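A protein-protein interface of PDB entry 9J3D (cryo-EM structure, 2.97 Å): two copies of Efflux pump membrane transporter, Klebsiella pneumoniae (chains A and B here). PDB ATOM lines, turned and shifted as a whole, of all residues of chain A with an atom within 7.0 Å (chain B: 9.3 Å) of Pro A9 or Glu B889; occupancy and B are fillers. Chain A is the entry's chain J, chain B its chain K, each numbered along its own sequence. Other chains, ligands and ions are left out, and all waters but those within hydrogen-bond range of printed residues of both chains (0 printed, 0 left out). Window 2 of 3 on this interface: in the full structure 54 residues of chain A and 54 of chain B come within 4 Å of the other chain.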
ATOM      1  N   PHE A   4      12.097 -28.594  -7.624  1.00  0.00           N
ATOM      2  CA  PHE A   4      11.150 -27.665  -7.023  1.00  0.00           C
ATOM      3  C   PHE A   4      11.644 -27.190  -5.662  1.00  0.00           C
ATOM      4  O   PHE A   4      11.512 -26.009  -5.319  1.00  0.00           O
ATOM      5  CB  PHE A   4       9.784 -28.342  -6.914  1.00  0.00           C
ATOM      6  CG  PHE A   4       8.765 -27.548  -6.156  1.00  0.00           C
ATOM      7  CD1 PHE A   4       8.074 -26.517  -6.768  1.00  0.00           C
ATOM      8  CD2 PHE A   4       8.476 -27.852  -4.838  1.00  0.00           C
ATOM      9  CE1 PHE A   4       7.127 -25.791  -6.073  1.00  0.00           C
ATOM     10  CE2 PHE A   4       7.531 -27.131  -4.140  1.00  0.00           C
ATOM     11  CZ  PHE A   4       6.856 -26.099  -4.757  1.00  0.00           C
ATOM     12  N   PHE A   5      12.223 -28.098  -4.875  1.00  0.00           N
ATOM     13  CA  PHE A   5      12.768 -27.709  -3.579  1.00  0.00           C
ATOM     14  C   PHE A   5      14.105 -26.990  -3.720  1.00  0.00           C
ATOM     15  O   PHE A   5      14.466 -26.187  -2.852  1.00  0.00           O
ATOM     16  CB  PHE A   5      12.902 -28.938  -2.685  1.00  0.00           C
ATOM     17  CG  PHE A   5      11.583 -29.508  -2.251  1.00  0.00           C
ATOM     18  CD1 PHE A   5      10.934 -29.013  -1.133  1.00  0.00           C
ATOM     19  CD2 PHE A   5      10.986 -30.530  -2.968  1.00  0.00           C
ATOM     20  CE1 PHE A   5       9.719 -29.534  -0.733  1.00  0.00           C
ATOM     21  CE2 PHE A   5       9.770 -31.054  -2.575  1.00  0.00           C
ATOM     22  CZ  PHE A   5       9.136 -30.555  -1.455  1.00  0.00           C
ATOM     23  N   ILE A   6      14.854 -27.269  -4.788  1.00  0.00           N
ATOM     24  CA  ILE A   6      16.058 -26.491  -5.068  1.00  0.00           C
ATOM     25  C   ILE A   6      15.698 -25.030  -5.276  1.00  0.00           C
ATOM     26  O   ILE A   6      16.337 -24.128  -4.720  1.00  0.00           O
ATOM     27  CB  ILE A   6      16.802 -27.056  -6.291  1.00  0.00           C
ATOM     28  CG1 ILE A   6      17.122 -28.532  -6.100  1.00  0.00           C
ATOM     29  CG2 ILE A   6      18.086 -26.285  -6.530  1.00  0.00           C
ATOM     30  CD1 ILE A   6      17.846 -28.806  -4.828  1.00  0.00           C
ATOM     31  N   ARG A   7      14.663 -24.776  -6.074  1.00  0.00           N
ATOM     32  CA  ARG A   7      14.229 -23.407  -6.313  1.00  0.00           C
ATOM     33  C   ARG A   7      13.432 -22.835  -5.149  1.00  0.00           C
ATOM     34  O   ARG A   7      13.259 -21.614  -5.077  1.00  0.00           O
ATOM     35  CB  ARG A   7      13.408 -23.341  -7.600  1.00  0.00           C
ATOM     36  CG  ARG A   7      14.225 -23.632  -8.849  1.00  0.00           C
ATOM     37  CD  ARG A   7      13.396 -23.512 -10.114  1.00  0.00           C
ATOM     38  NE  ARG A   7      14.192 -23.792 -11.304  1.00  0.00           N
ATOM     39  CZ  ARG A   7      13.778 -23.590 -12.547  1.00  0.00           C
ATOM     40  NH1 ARG A   7      12.574 -23.107 -12.807  1.00  0.00           N
ATOM     41  NH2 ARG A   7      14.593 -23.883 -13.558  1.00  0.00           N
ATOM     42  N   ARG A   8      12.953 -23.680  -4.238  1.00  0.00           N
ATOM     43  CA  ARG A   8      12.166 -23.249  -3.082  1.00  0.00           C
ATOM     44  C   ARG A   8      12.708 -23.915  -1.823  1.00  0.00           C
ATOM     45  O   ARG A   8      12.124 -24.877  -1.311  1.00  0.00           O
ATOM     46  CB  ARG A   8      10.685 -23.571  -3.282  1.00  0.00           C
ATOM     47  CG  ARG A   8      10.062 -22.869  -4.475  1.00  0.00           C
ATOM     48  CD  ARG A   8       8.555 -23.032  -4.491  1.00  0.00           C
ATOM     49  NE  ARG A   8       7.950 -22.366  -5.638  1.00  0.00           N
ATOM     50  CZ  ARG A   8       6.655 -22.110  -5.758  1.00  0.00           C
ATOM     51  NH1 ARG A   8       5.792 -22.455  -4.816  1.00  0.00           N
ATOM     52  NH2 ARG A   8       6.214 -21.494  -6.851  1.00  0.00           N
ATOM     53  N   PRO A   9      13.832 -23.425  -1.297  1.00  0.00           N
ATOM     54  CA  PRO A   9      14.416 -24.061  -0.104  1.00  0.00           C
ATOM     55  C   PRO A   9      13.600 -23.867   1.164  1.00  0.00           C
ATOM     56  O   PRO A   9      13.524 -24.792   1.988  1.00  0.00           O
ATOM     57  CB  PRO A   9      15.789 -23.387   0.004  1.00  0.00           C
ATOM     58  CG  PRO A   9      15.610 -22.067  -0.664  1.00  0.00           C
ATOM     59  CD  PRO A   9      14.660 -22.315  -1.797  1.00  0.00           C
ATOM     60  N   ASN A  10      12.998 -22.692   1.356  1.00  0.00           N
ATOM     61  CA  ASN A  10      12.248 -22.447   2.584  1.00  0.00           C
ATOM     62  C   ASN A  10      11.055 -23.385   2.696  1.00  0.00           C
ATOM     63  O   ASN A  10      10.635 -23.732   3.804  1.00  0.00           O
ATOM     64  CB  ASN A  10      11.801 -20.989   2.651  1.00  0.00           C
ATOM     65  CG  ASN A  10      12.967 -20.026   2.738  1.00  0.00           C
ATOM     66  OD1 ASN A  10      14.121 -20.442   2.849  1.00  0.00           O
ATOM     67  ND2 ASN A  10      12.674 -18.733   2.690  1.00  0.00           N
ATOM     68  N   PHE A  11      10.499 -23.818   1.563  1.00  0.00           N
ATOM     69  CA  PHE A  11       9.428 -24.809   1.601  1.00  0.00           C
ATOM     70  C   PHE A  11       9.923 -26.127   2.188  1.00  0.00           C
ATOM     71  O   PHE A  11       9.245 -26.737   3.028  1.00  0.00           O
ATOM     72  CB  PHE A  11       8.870 -25.017   0.192  1.00  0.00           C
ATOM     73  CG  PHE A  11       7.533 -25.708   0.153  1.00  0.00           C
ATOM     74  CD1 PHE A  11       6.956 -26.038  -1.058  1.00  0.00           C
ATOM     75  CD2 PHE A  11       6.847 -26.010   1.315  1.00  0.00           C
ATOM     76  CE1 PHE A  11       5.730 -26.668  -1.113  1.00  0.00           C
ATOM     77  CE2 PHE A  11       5.620 -26.643   1.269  1.00  0.00           C
ATOM     78  CZ  PHE A  11       5.060 -26.971   0.052  1.00  0.00           C
ATOM     79  N   ALA A  12      11.104 -26.580   1.764  1.00  0.00           N
ATOM     80  CA  ALA A  12      11.680 -27.788   2.343  1.00  0.00           C
ATOM     81  C   ALA A  12      11.961 -27.598   3.826  1.00  0.00           C
ATOM     82  O   ALA A  12      11.716 -28.502   4.636  1.00  0.00           O
ATOM     83  CB  ALA A  12      12.958 -28.172   1.601  1.00  0.00           C
ATOM     84  N   TRP A  13      12.470 -26.424   4.200  1.00  0.00           N
ATOM     85  CA  TRP A  13      12.714 -26.148   5.611  1.00  0.00           C
ATOM     86  C   TRP A  13      11.421 -26.204   6.416  1.00  0.00           C
ATOM     87  O   TRP A  13      11.410 -26.686   7.553  1.00  0.00           O
ATOM     88  CB  TRP A  13      13.386 -24.787   5.772  1.00  0.00           C
ATOM     89  CG  TRP A  13      14.854 -24.802   5.489  1.00  0.00           C
ATOM     90  CD1 TRP A  13      15.472 -24.385   4.348  1.00  0.00           C
ATOM     91  CD2 TRP A  13      15.891 -25.251   6.367  1.00  0.00           C
ATOM     92  NE1 TRP A  13      16.832 -24.547   4.460  1.00  0.00           N
ATOM     93  CE2 TRP A  13      17.114 -25.078   5.691  1.00  0.00           C
ATOM     94  CE3 TRP A  13      15.904 -25.784   7.659  1.00  0.00           C
ATOM     95  CZ2 TRP A  13      18.336 -25.418   6.262  1.00  0.00           C
ATOM     96  CZ3 TRP A  13      17.118 -26.121   8.222  1.00  0.00           C
ATOM     97  CH2 TRP A  13      18.318 -25.937   7.526  1.00  0.00           C
ATOM     98  N   VAL A  14      10.321 -25.715   5.845  1.00  0.00           N
ATOM     99  CA  VAL A  14       9.051 -25.709   6.566  1.00  0.00           C
ATOM    100  C   VAL A  14       8.506 -27.125   6.704  1.00  0.00           C
ATOM    101  O   VAL A  14       7.958 -27.495   7.747  1.00  0.00           O
ATOM    102  CB  VAL A  14       8.037 -24.783   5.875  1.00  0.00           C
ATOM    103  CG1 VAL A  14       6.653 -25.017   6.450  1.00  0.00           C
ATOM    104  CG2 VAL A  14       8.447 -23.336   6.051  1.00  0.00           C
ATOM    105  N   VAL A  15       8.622 -27.933   5.649  1.00  0.00           N
ATOM    106  CA  VAL A  15       8.195 -29.332   5.747  1.00  0.00           C
ATOM    107  C   VAL A  15       8.994 -30.045   6.827  1.00  0.00           C
ATOM    108  O   VAL A  15       8.478 -30.842   7.621  1.00  0.00           O
ATOM    109  CB  VAL A  15       8.338 -30.035   4.387  1.00  0.00           C
ATOM    110  CG1 VAL A  15       8.010 -31.514   4.519  1.00  0.00           C
ATOM    111  CG2 VAL A  15       7.425 -29.379   3.363  1.00  0.00           C
ATOM    112  N   PHE A 490      14.166 -32.931   1.581  1.00  0.00           N
ATOM    113  CA  PHE A 490      15.090 -32.146   2.395  1.00  0.00           C
ATOM    114  C   PHE A 490      16.460 -31.993   1.751  1.00  0.00           C
ATOM    115  O   PHE A 490      16.863 -30.881   1.395  1.00  0.00           O
ATOM    116  CB  PHE A 490      15.294 -32.802   3.753  1.00  0.00           C
ATOM    117  CG  PHE A 490      15.312 -31.847   4.897  1.00  0.00           C
ATOM    118  CD1 PHE A 490      16.205 -30.796   4.935  1.00  0.00           C
ATOM    119  CD2 PHE A 490      14.555 -32.076   5.985  1.00  0.00           C
ATOM    120  CE1 PHE A 490      16.256 -29.941   6.013  1.00  0.00           C
ATOM    121  CE2 PHE A 490      14.687 -31.325   7.051  1.00  0.00           C
ATOM    122  CZ  PHE A 490      15.485 -30.202   7.053  1.00  0.00           C
ATOM    123  N   ALA A 493      17.687 -29.606  -1.031  1.00  0.00           N
ATOM    124  CA  ALA A 493      17.624 -28.218  -0.585  1.00  0.00           C
ATOM    125  C   ALA A 493      18.775 -27.889   0.356  1.00  0.00           C
ATOM    126  O   ALA A 493      19.322 -26.781   0.313  1.00  0.00           O
ATOM    127  CB  ALA A 493      16.284 -27.944   0.093  1.00  0.00           C
ATOM    128  N   LEU A 494      19.152 -28.836   1.216  1.00  0.00           N
ATOM    129  CA  LEU A 494      20.284 -28.608   2.107  1.00  0.00           C
ATOM    130  C   LEU A 494      21.574 -28.400   1.325  1.00  0.00           C
ATOM    131  O   LEU A 494      22.373 -27.521   1.661  1.00  0.00           O
ATOM    132  CB  LEU A 494      20.433 -29.776   3.079  1.00  0.00           C
ATOM    133  CG  LEU A 494      19.460 -29.784   4.258  1.00  0.00           C
ATOM    134  CD1 LEU A 494      19.658 -31.024   5.117  1.00  0.00           C
ATOM    135  CD2 LEU A 494      19.631 -28.524   5.085  1.00  0.00           C
ATOM    136  N   ALA A 496      21.715 -27.313  -1.770  1.00  0.00           N
ATOM    137  CA  ALA A 496      21.559 -26.053  -2.484  1.00  0.00           C
ATOM    138  C   ALA A 496      21.780 -24.845  -1.584  1.00  0.00           C
ATOM    139  O   ALA A 496      22.196 -23.789  -2.074  1.00  0.00           O
ATOM    140  CB  ALA A 496      20.172 -25.980  -3.122  1.00  0.00           C
ATOM    141  N   THR A 497      21.512 -24.971  -0.287  1.00  0.00           N
ATOM    142  CA  THR A 497      21.607 -23.842   0.630  1.00  0.00           C
ATOM    143  C   THR A 497      22.918 -23.761   1.397  1.00  0.00           C
ATOM    144  O   THR A 497      23.553 -22.705   1.390  1.00  0.00           O
ATOM    145  CB  THR A 497      20.459 -23.885   1.645  1.00  0.00           C
ATOM    146  OG1 THR A 497      20.282 -25.229   2.111  1.00  0.00           O
ATOM    147  CG2 THR A 497      19.175 -23.403   1.009  1.00  0.00           C
ATOM    148  N   PHE B 881       2.389 -19.396  11.821  1.00  0.00           N
ATOM    149  CA  PHE B 881       3.686 -18.878  11.398  1.00  0.00           C
ATOM    150  C   PHE B 881       4.360 -19.818  10.407  1.00  0.00           C
ATOM    151  O   PHE B 881       4.884 -19.382   9.372  1.00  0.00           O
ATOM    152  CB  PHE B 881       4.582 -18.648  12.613  1.00  0.00           C
ATOM    153  CG  PHE B 881       5.989 -18.258  12.263  1.00  0.00           C
ATOM    154  CD1 PHE B 881       6.234 -17.178  11.441  1.00  0.00           C
ATOM    155  CD2 PHE B 881       7.066 -18.951  12.782  1.00  0.00           C
ATOM    156  CE1 PHE B 881       7.519 -16.799  11.127  1.00  0.00           C
ATOM    157  CE2 PHE B 881       8.359 -18.578  12.469  1.00  0.00           C
ATOM    158  CZ  PHE B 881       8.581 -17.498  11.641  1.00  0.00           C
ATOM    159  N   LEU B 882       4.356 -21.119  10.712  1.00  0.00           N
ATOM    160  CA  LEU B 882       5.009 -22.080   9.829  1.00  0.00           C
ATOM    161  C   LEU B 882       4.339 -22.132   8.461  1.00  0.00           C
ATOM    162  O   LEU B 882       5.017 -22.180   7.428  1.00  0.00           O
ATOM    163  CB  LEU B 882       5.027 -23.463  10.475  1.00  0.00           C
ATOM    164  CG  LEU B 882       6.389 -23.833  11.057  1.00  0.00           C
ATOM    165  CD1 LEU B 882       7.428 -23.791   9.952  1.00  0.00           C
ATOM    166  CD2 LEU B 882       6.766 -22.894  12.188  1.00  0.00           C
ATOM    167  N   LEU B 883       3.008 -22.119   8.428  1.00  0.00           N
ATOM    168  CA  LEU B 883       2.331 -22.169   7.137  1.00  0.00           C
ATOM    169  C   LEU B 883       2.610 -20.918   6.322  1.00  0.00           C
ATOM    170  O   LEU B 883       2.742 -20.980   5.093  1.00  0.00           O
ATOM    171  CB  LEU B 883       0.836 -22.351   7.341  1.00  0.00           C
ATOM    172  CG  LEU B 883       0.545 -23.647   8.081  1.00  0.00           C
ATOM    173  CD1 LEU B 883      -0.931 -23.763   8.314  1.00  0.00           C
ATOM    174  CD2 LEU B 883       1.091 -24.846   7.323  1.00  0.00           C
ATOM    175  N   LEU B 884       2.692 -19.774   7.011  1.00  0.00           N
ATOM    176  CA  LEU B 884       2.925 -18.479   6.315  1.00  0.00           C
ATOM    177  C   LEU B 884       4.326 -18.478   5.695  1.00  0.00           C
ATOM    178  O   LEU B 884       4.447 -18.079   4.522  1.00  0.00           O
ATOM    179  CB  LEU B 884       2.770 -17.333   7.319  1.00  0.00           C
ATOM    180  CG  LEU B 884       1.704 -16.298   6.967  1.00  0.00           C
ATOM    181  CD1 LEU B 884       0.775 -16.823   5.884  1.00  0.00           C
ATOM    182  CD2 LEU B 884       0.911 -15.900   8.202  1.00  0.00           C
ATOM    183  N   VAL B 885       5.338 -18.901   6.460  1.00  0.00           N
ATOM    184  CA  VAL B 885       6.699 -18.956   5.916  1.00  0.00           C
ATOM    185  C   VAL B 885       6.777 -19.991   4.800  1.00  0.00           C
ATOM    186  O   VAL B 885       7.557 -19.849   3.850  1.00  0.00           O
ATOM    187  CB  VAL B 885       7.738 -19.216   7.027  1.00  0.00           C
ATOM    188  CG1 VAL B 885       7.394 -20.427   7.833  1.00  0.00           C
ATOM    189  CG2 VAL B 885       9.136 -19.382   6.442  1.00  0.00           C
ATOM    190  N   ALA B 886       5.955 -21.040   4.883  1.00  0.00           N
ATOM    191  CA  ALA B 886       5.861 -21.975   3.766  1.00  0.00           C
ATOM    192  C   ALA B 886       5.349 -21.289   2.508  1.00  0.00           C
ATOM    193  O   ALA B 886       5.909 -21.469   1.422  1.00  0.00           O
ATOM    194  CB  ALA B 886       4.943 -23.139   4.125  1.00  0.00           C
ATOM    195  N   LEU B 887       4.282 -20.501   2.637  1.00  0.00           N
ATOM    196  CA  LEU B 887       3.644 -19.945   1.449  1.00  0.00           C
ATOM    197  C   LEU B 887       4.495 -18.844   0.824  1.00  0.00           C
ATOM    198  O   LEU B 887       4.658 -18.802  -0.401  1.00  0.00           O
ATOM    199  CB  LEU B 887       2.242 -19.436   1.801  1.00  0.00           C
ATOM    200  CG  LEU B 887       1.215 -19.043   0.725  1.00  0.00           C
ATOM    201  CD1 LEU B 887       1.605 -17.846  -0.135  1.00  0.00           C
ATOM    202  CD2 LEU B 887       0.931 -20.248  -0.165  1.00  0.00           C
ATOM    203  N   TYR B 888       5.053 -17.947   1.640  1.00  0.00           N
ATOM    204  CA  TYR B 888       5.724 -16.766   1.107  1.00  0.00           C
ATOM    205  C   TYR B 888       7.193 -16.980   0.767  1.00  0.00           C
ATOM    206  O   TYR B 888       7.821 -16.061   0.229  1.00  0.00           O
ATOM    207  CB  TYR B 888       5.594 -15.590   2.078  1.00  0.00           C
ATOM    208  CG  TYR B 888       4.177 -15.114   2.235  1.00  0.00           C
ATOM    209  CD1 TYR B 888       3.684 -14.736   3.454  1.00  0.00           C
ATOM    210  CD2 TYR B 888       3.323 -15.066   1.150  1.00  0.00           C
ATOM    211  CE1 TYR B 888       2.405 -14.269   3.576  1.00  0.00           C
ATOM    212  CE2 TYR B 888       2.017 -14.639   1.282  1.00  0.00           C
ATOM    213  CZ  TYR B 888       1.558 -14.267   2.505  1.00  0.00           C
ATOM    214  OH  TYR B 888       0.261 -13.834   2.660  1.00  0.00           O
ATOM    215  N   GLU B 889       7.754 -18.155   1.052  1.00  0.00           N
ATOM    216  CA  GLU B 889       9.169 -18.428   0.796  1.00  0.00           C
ATOM    217  C   GLU B 889      10.047 -17.364   1.449  1.00  0.00           C
ATOM    218  O   GLU B 889      11.037 -16.901   0.881  1.00  0.00           O
ATOM    219  CB  GLU B 889       9.446 -18.526  -0.707  1.00  0.00           C
ATOM    220  CG  GLU B 889      10.209 -19.777  -1.150  1.00  0.00           C
ATOM    221  CD  GLU B 889      11.644 -19.827  -0.660  1.00  0.00           C
ATOM    222  OE1 GLU B 889      12.154 -20.945  -0.442  1.00  0.00           O
ATOM    223  OE2 GLU B 889      12.276 -18.761  -0.523  1.00  0.00           O
ATOM    224  N   SER B 890       9.658 -16.953   2.652  1.00  0.00           N
ATOM    225  CA  SER B 890      10.355 -15.903   3.377  1.00  0.00           C
ATOM    226  C   SER B 890       9.947 -15.967   4.837  1.00  0.00           C
ATOM    227  O   SER B 890       8.931 -16.578   5.174  1.00  0.00           O
ATOM    228  CB  SER B 890      10.037 -14.520   2.799  1.00  0.00           C
ATOM    229  OG  SER B 890      10.625 -13.494   3.578  1.00  0.00           O
ATOM    230  N   TRP B 891      10.743 -15.337   5.699  1.00  0.00           N
ATOM    231  CA  TRP B 891      10.399 -15.211   7.109  1.00  0.00           C
ATOM    232  C   TRP B 891       9.905 -13.813   7.453  1.00  0.00           C
ATOM    233  O   TRP B 891       8.975 -13.663   8.262  1.00  0.00           O
ATOM    234  CB  TRP B 891      11.613 -15.561   7.976  1.00  0.00           C
ATOM    235  CG  TRP B 891      12.136 -16.955   7.755  1.00  0.00           C
ATOM    236  CD1 TRP B 891      13.022 -17.354   6.800  1.00  0.00           C
ATOM    237  CD2 TRP B 891      11.818 -18.128   8.518  1.00  0.00           C
ATOM    238  NE1 TRP B 891      13.268 -18.702   6.911  1.00  0.00           N
ATOM    239  CE2 TRP B 891      12.540 -19.200   7.959  1.00  0.00           C
ATOM    240  CE3 TRP B 891      10.988 -18.375   9.614  1.00  0.00           C
ATOM    241  CZ2 TRP B 891      12.458 -20.498   8.460  1.00  0.00           C
ATOM    242  CZ3 TRP B 891      10.907 -19.664  10.110  1.00  0.00           C
ATOM    243  CH2 TRP B 891      11.639 -20.708   9.534  1.00  0.00           C
ATOM    244  N   ALA B 892      10.488 -12.791   6.820  1.00  0.00           N
ATOM    245  CA  ALA B 892      10.149 -11.406   7.115  1.00  0.00           C
ATOM    246  C   ALA B 892       8.691 -11.096   6.805  1.00  0.00           C
ATOM    247  O   ALA B 892       8.021 -10.423   7.594  1.00  0.00           O
ATOM    248  CB  ALA B 892      11.067 -10.467   6.336  1.00  0.00           C
ATOM    249  N   ILE B 893       8.192 -11.555   5.662  1.00  0.00           N
ATOM    250  CA  ILE B 893       6.795 -11.340   5.286  1.00  0.00           C
ATOM    251  C   ILE B 893       5.889 -12.018   6.310  1.00  0.00           C
ATOM    252  O   ILE B 893       4.874 -11.425   6.718  1.00  0.00           O
ATOM    253  CB  ILE B 893       6.517 -11.833   3.855  1.00  0.00           C
ATOM    254  CG1 ILE B 893       7.513 -11.210   2.878  1.00  0.00           C
ATOM    255  CG2 ILE B 893       5.092 -11.507   3.444  1.00  0.00           C
ATOM    256  CD1 ILE B 893       7.412 -11.760   1.472  1.00  0.00           C
ATOM    257  N   PRO B 894       6.176 -13.257   6.733  1.00  0.00           N
ATOM    258  CA  PRO B 894       5.384 -13.830   7.828  1.00  0.00           C
ATOM    259  C   PRO B 894       5.393 -13.046   9.121  1.00  0.00           C
ATOM    260  O   PRO B 894       4.324 -12.909   9.726  1.00  0.00           O
ATOM    261  CB  PRO B 894       5.981 -15.233   7.986  1.00  0.00           C
ATOM    262  CG  PRO B 894       6.377 -15.574   6.626  1.00  0.00           C
ATOM    263  CD  PRO B 894       6.940 -14.315   6.048  1.00  0.00           C
ATOM    264  N   LYS B 946       3.656  -8.046  -1.943  1.00  0.00           N
ATOM    265  CA  LYS B 946       4.828  -8.819  -2.337  1.00  0.00           C
ATOM    266  C   LYS B 946       4.921  -8.939  -3.851  1.00  0.00           C
ATOM    267  O   LYS B 946       6.013  -8.849  -4.426  1.00  0.00           O
ATOM    268  CB  LYS B 946       4.776 -10.201  -1.683  1.00  0.00           C
ATOM    269  CG  LYS B 946       5.966 -11.093  -1.977  1.00  0.00           C
ATOM    270  CD  LYS B 946       5.566 -12.557  -1.904  1.00  0.00           C
ATOM    271  CE  LYS B 946       6.696 -13.469  -2.350  1.00  0.00           C
ATOM    272  NZ  LYS B 946       6.228 -14.865  -2.570  1.00  0.00           N
ATOM    273  N   GLU B 950       8.035  -7.398  -5.933  1.00  0.00           N
ATOM    274  CA  GLU B 950       8.878  -8.200  -6.813  1.00  0.00           C
ATOM    275  C   GLU B 950       8.865  -7.670  -8.239  1.00  0.00           C
ATOM    276  O   GLU B 950       9.715  -8.054  -9.049  1.00  0.00           O
ATOM    277  CB  GLU B 950       8.430  -9.660  -6.790  1.00  0.00           C
ATOM    278  CG  GLU B 950       8.788 -10.406  -5.518  1.00  0.00           C
ATOM    279  CD  GLU B 950       8.304 -11.840  -5.532  1.00  0.00           C
ATOM    280  OE1 GLU B 950       7.487 -12.184  -6.412  1.00  0.00           O
ATOM    281  OE2 GLU B 950       8.744 -12.626  -4.668  1.00  0.00           O
ATOM    282  N   THR B1030      15.144  -6.468   3.707  1.00  0.00           N
ATOM    283  CA  THR B1030      14.790  -7.524   2.769  1.00  0.00           C
ATOM    284  C   THR B1030      14.889  -7.025   1.332  1.00  0.00           C
ATOM    285  O   THR B1030      14.568  -5.871   1.033  1.00  0.00           O
ATOM    286  CB  THR B1030      13.376  -8.031   3.052  1.00  0.00           C
ATOM    287  OG1 THR B1030      13.170  -8.106   4.468  1.00  0.00           O
ATOM    288  CG2 THR B1030      13.170  -9.408   2.444  1.00  0.00           C
ATOM    289  N   LYS B1031      15.341  -7.915   0.431  1.00  0.00           N
ATOM    290  CA  LYS B1031      15.522  -7.650  -0.986  1.00  0.00           C
ATOM    291  C   LYS B1031      14.501  -8.422  -1.814  1.00  0.00           C
ATOM    292  O   LYS B1031      14.037  -9.489  -1.401  1.00  0.00           O
ATOM    293  CB  LYS B1031      16.937  -8.038  -1.429  1.00  0.00           C
ATOM    294  CG  LYS B1031      18.023  -7.112  -0.906  1.00  0.00           C
ATOM    295  CD  LYS B1031      19.380  -7.464  -1.493  1.00  0.00           C
ATOM    296  CE  LYS B1031      20.453  -6.498  -1.017  1.00  0.00           C
ATOM    297  NZ  LYS B1031      21.783  -6.813  -1.609  1.00  0.00           N
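N of Ala B892 is in hydrogen-bond range of OG of Ser B890 (3.3 Å).
OE1 of Glu B889 touches C of Arg A8, 3.3 Å away.
ND2 of Asn A10 touches N of Ser B890, 3.5 Å away.
Glu B889 touches Phe A11 (OE1 to N, 3.9 Å).
Val A14 touches Leu B882 (CG1 to O, 3.4 Å).
Val A14 touches Val B885 (CG2 to CG1, 3.6 Å).
Val A14 touches Ala B886 (CG1 to CB, 3.4 Å).
The side-chain carboxylate (OE1) of Glu B889 lies close to the backbone nitrogen (N) of Pro A9, 3.1 Å away.
The backbone NH (N) of Asn A10 is in hydrogen-bond range of the side-chain carboxylate (OE1) of Glu B889 (2.6 Å).
Of the 18 printed residues of chain B, 5 touch a printed residue of chain A.
Hydrophobic or aromatic side chains of chain B that line the printed part of chain A: Leu B882, Val B885 and Ala B886.
Printed residues of chain A that touch a printed residue of chain B: Arg A8, Pro A9, Asn A10, Phe A11 and Val A14.
Hydrophobic or aromatic side chains of chain A within 4 Å of the printed part of chain B: Pro A9 and Val A14.
Among the printed residues, 8 pairs touch across the chains.
Among the printed residues, no Asp or Glu carboxylate lies within 4 Å of a Lys or Arg side-chain nitrogen of the other chain.
No position is printed for both chains.
Of the 8 pairs that touch across the chains among the printed residues, none has its exchanged pair printed and touching as well.
Of the printed residues of chain B, Pro A9 touches Glu B889.
Of chain A, only Arg A8, Pro A9, Asn A10 and Phe A11 come within 4 Å of Glu B889.
Asn A10 touches just these residues of chain B: Glu B889 and Ser B890.
No residue of chain B comes within 4 Å of Ala A12.
Of the printed residues of chain B, Val A14 touches Leu B882, Val B885 and Ala B886.
Printed residues of chain B within 4 Å of Phe A11: Glu B889.
Printed residues of chain A within 4 Å of Leu B882: Val A14.
Printed residues of chain A within 4 Å of Ser B890: Asn A10 (3.5 Å).
Of the printed residues of chain A, Val B885 touches Val A14.
The nearest printed residue of chain B that does not touch Pro A9 is Trp B891 (7.7 Å).
The nearest residue of chain A that does not touch Glu B889 is Arg A7 (4.8 Å).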
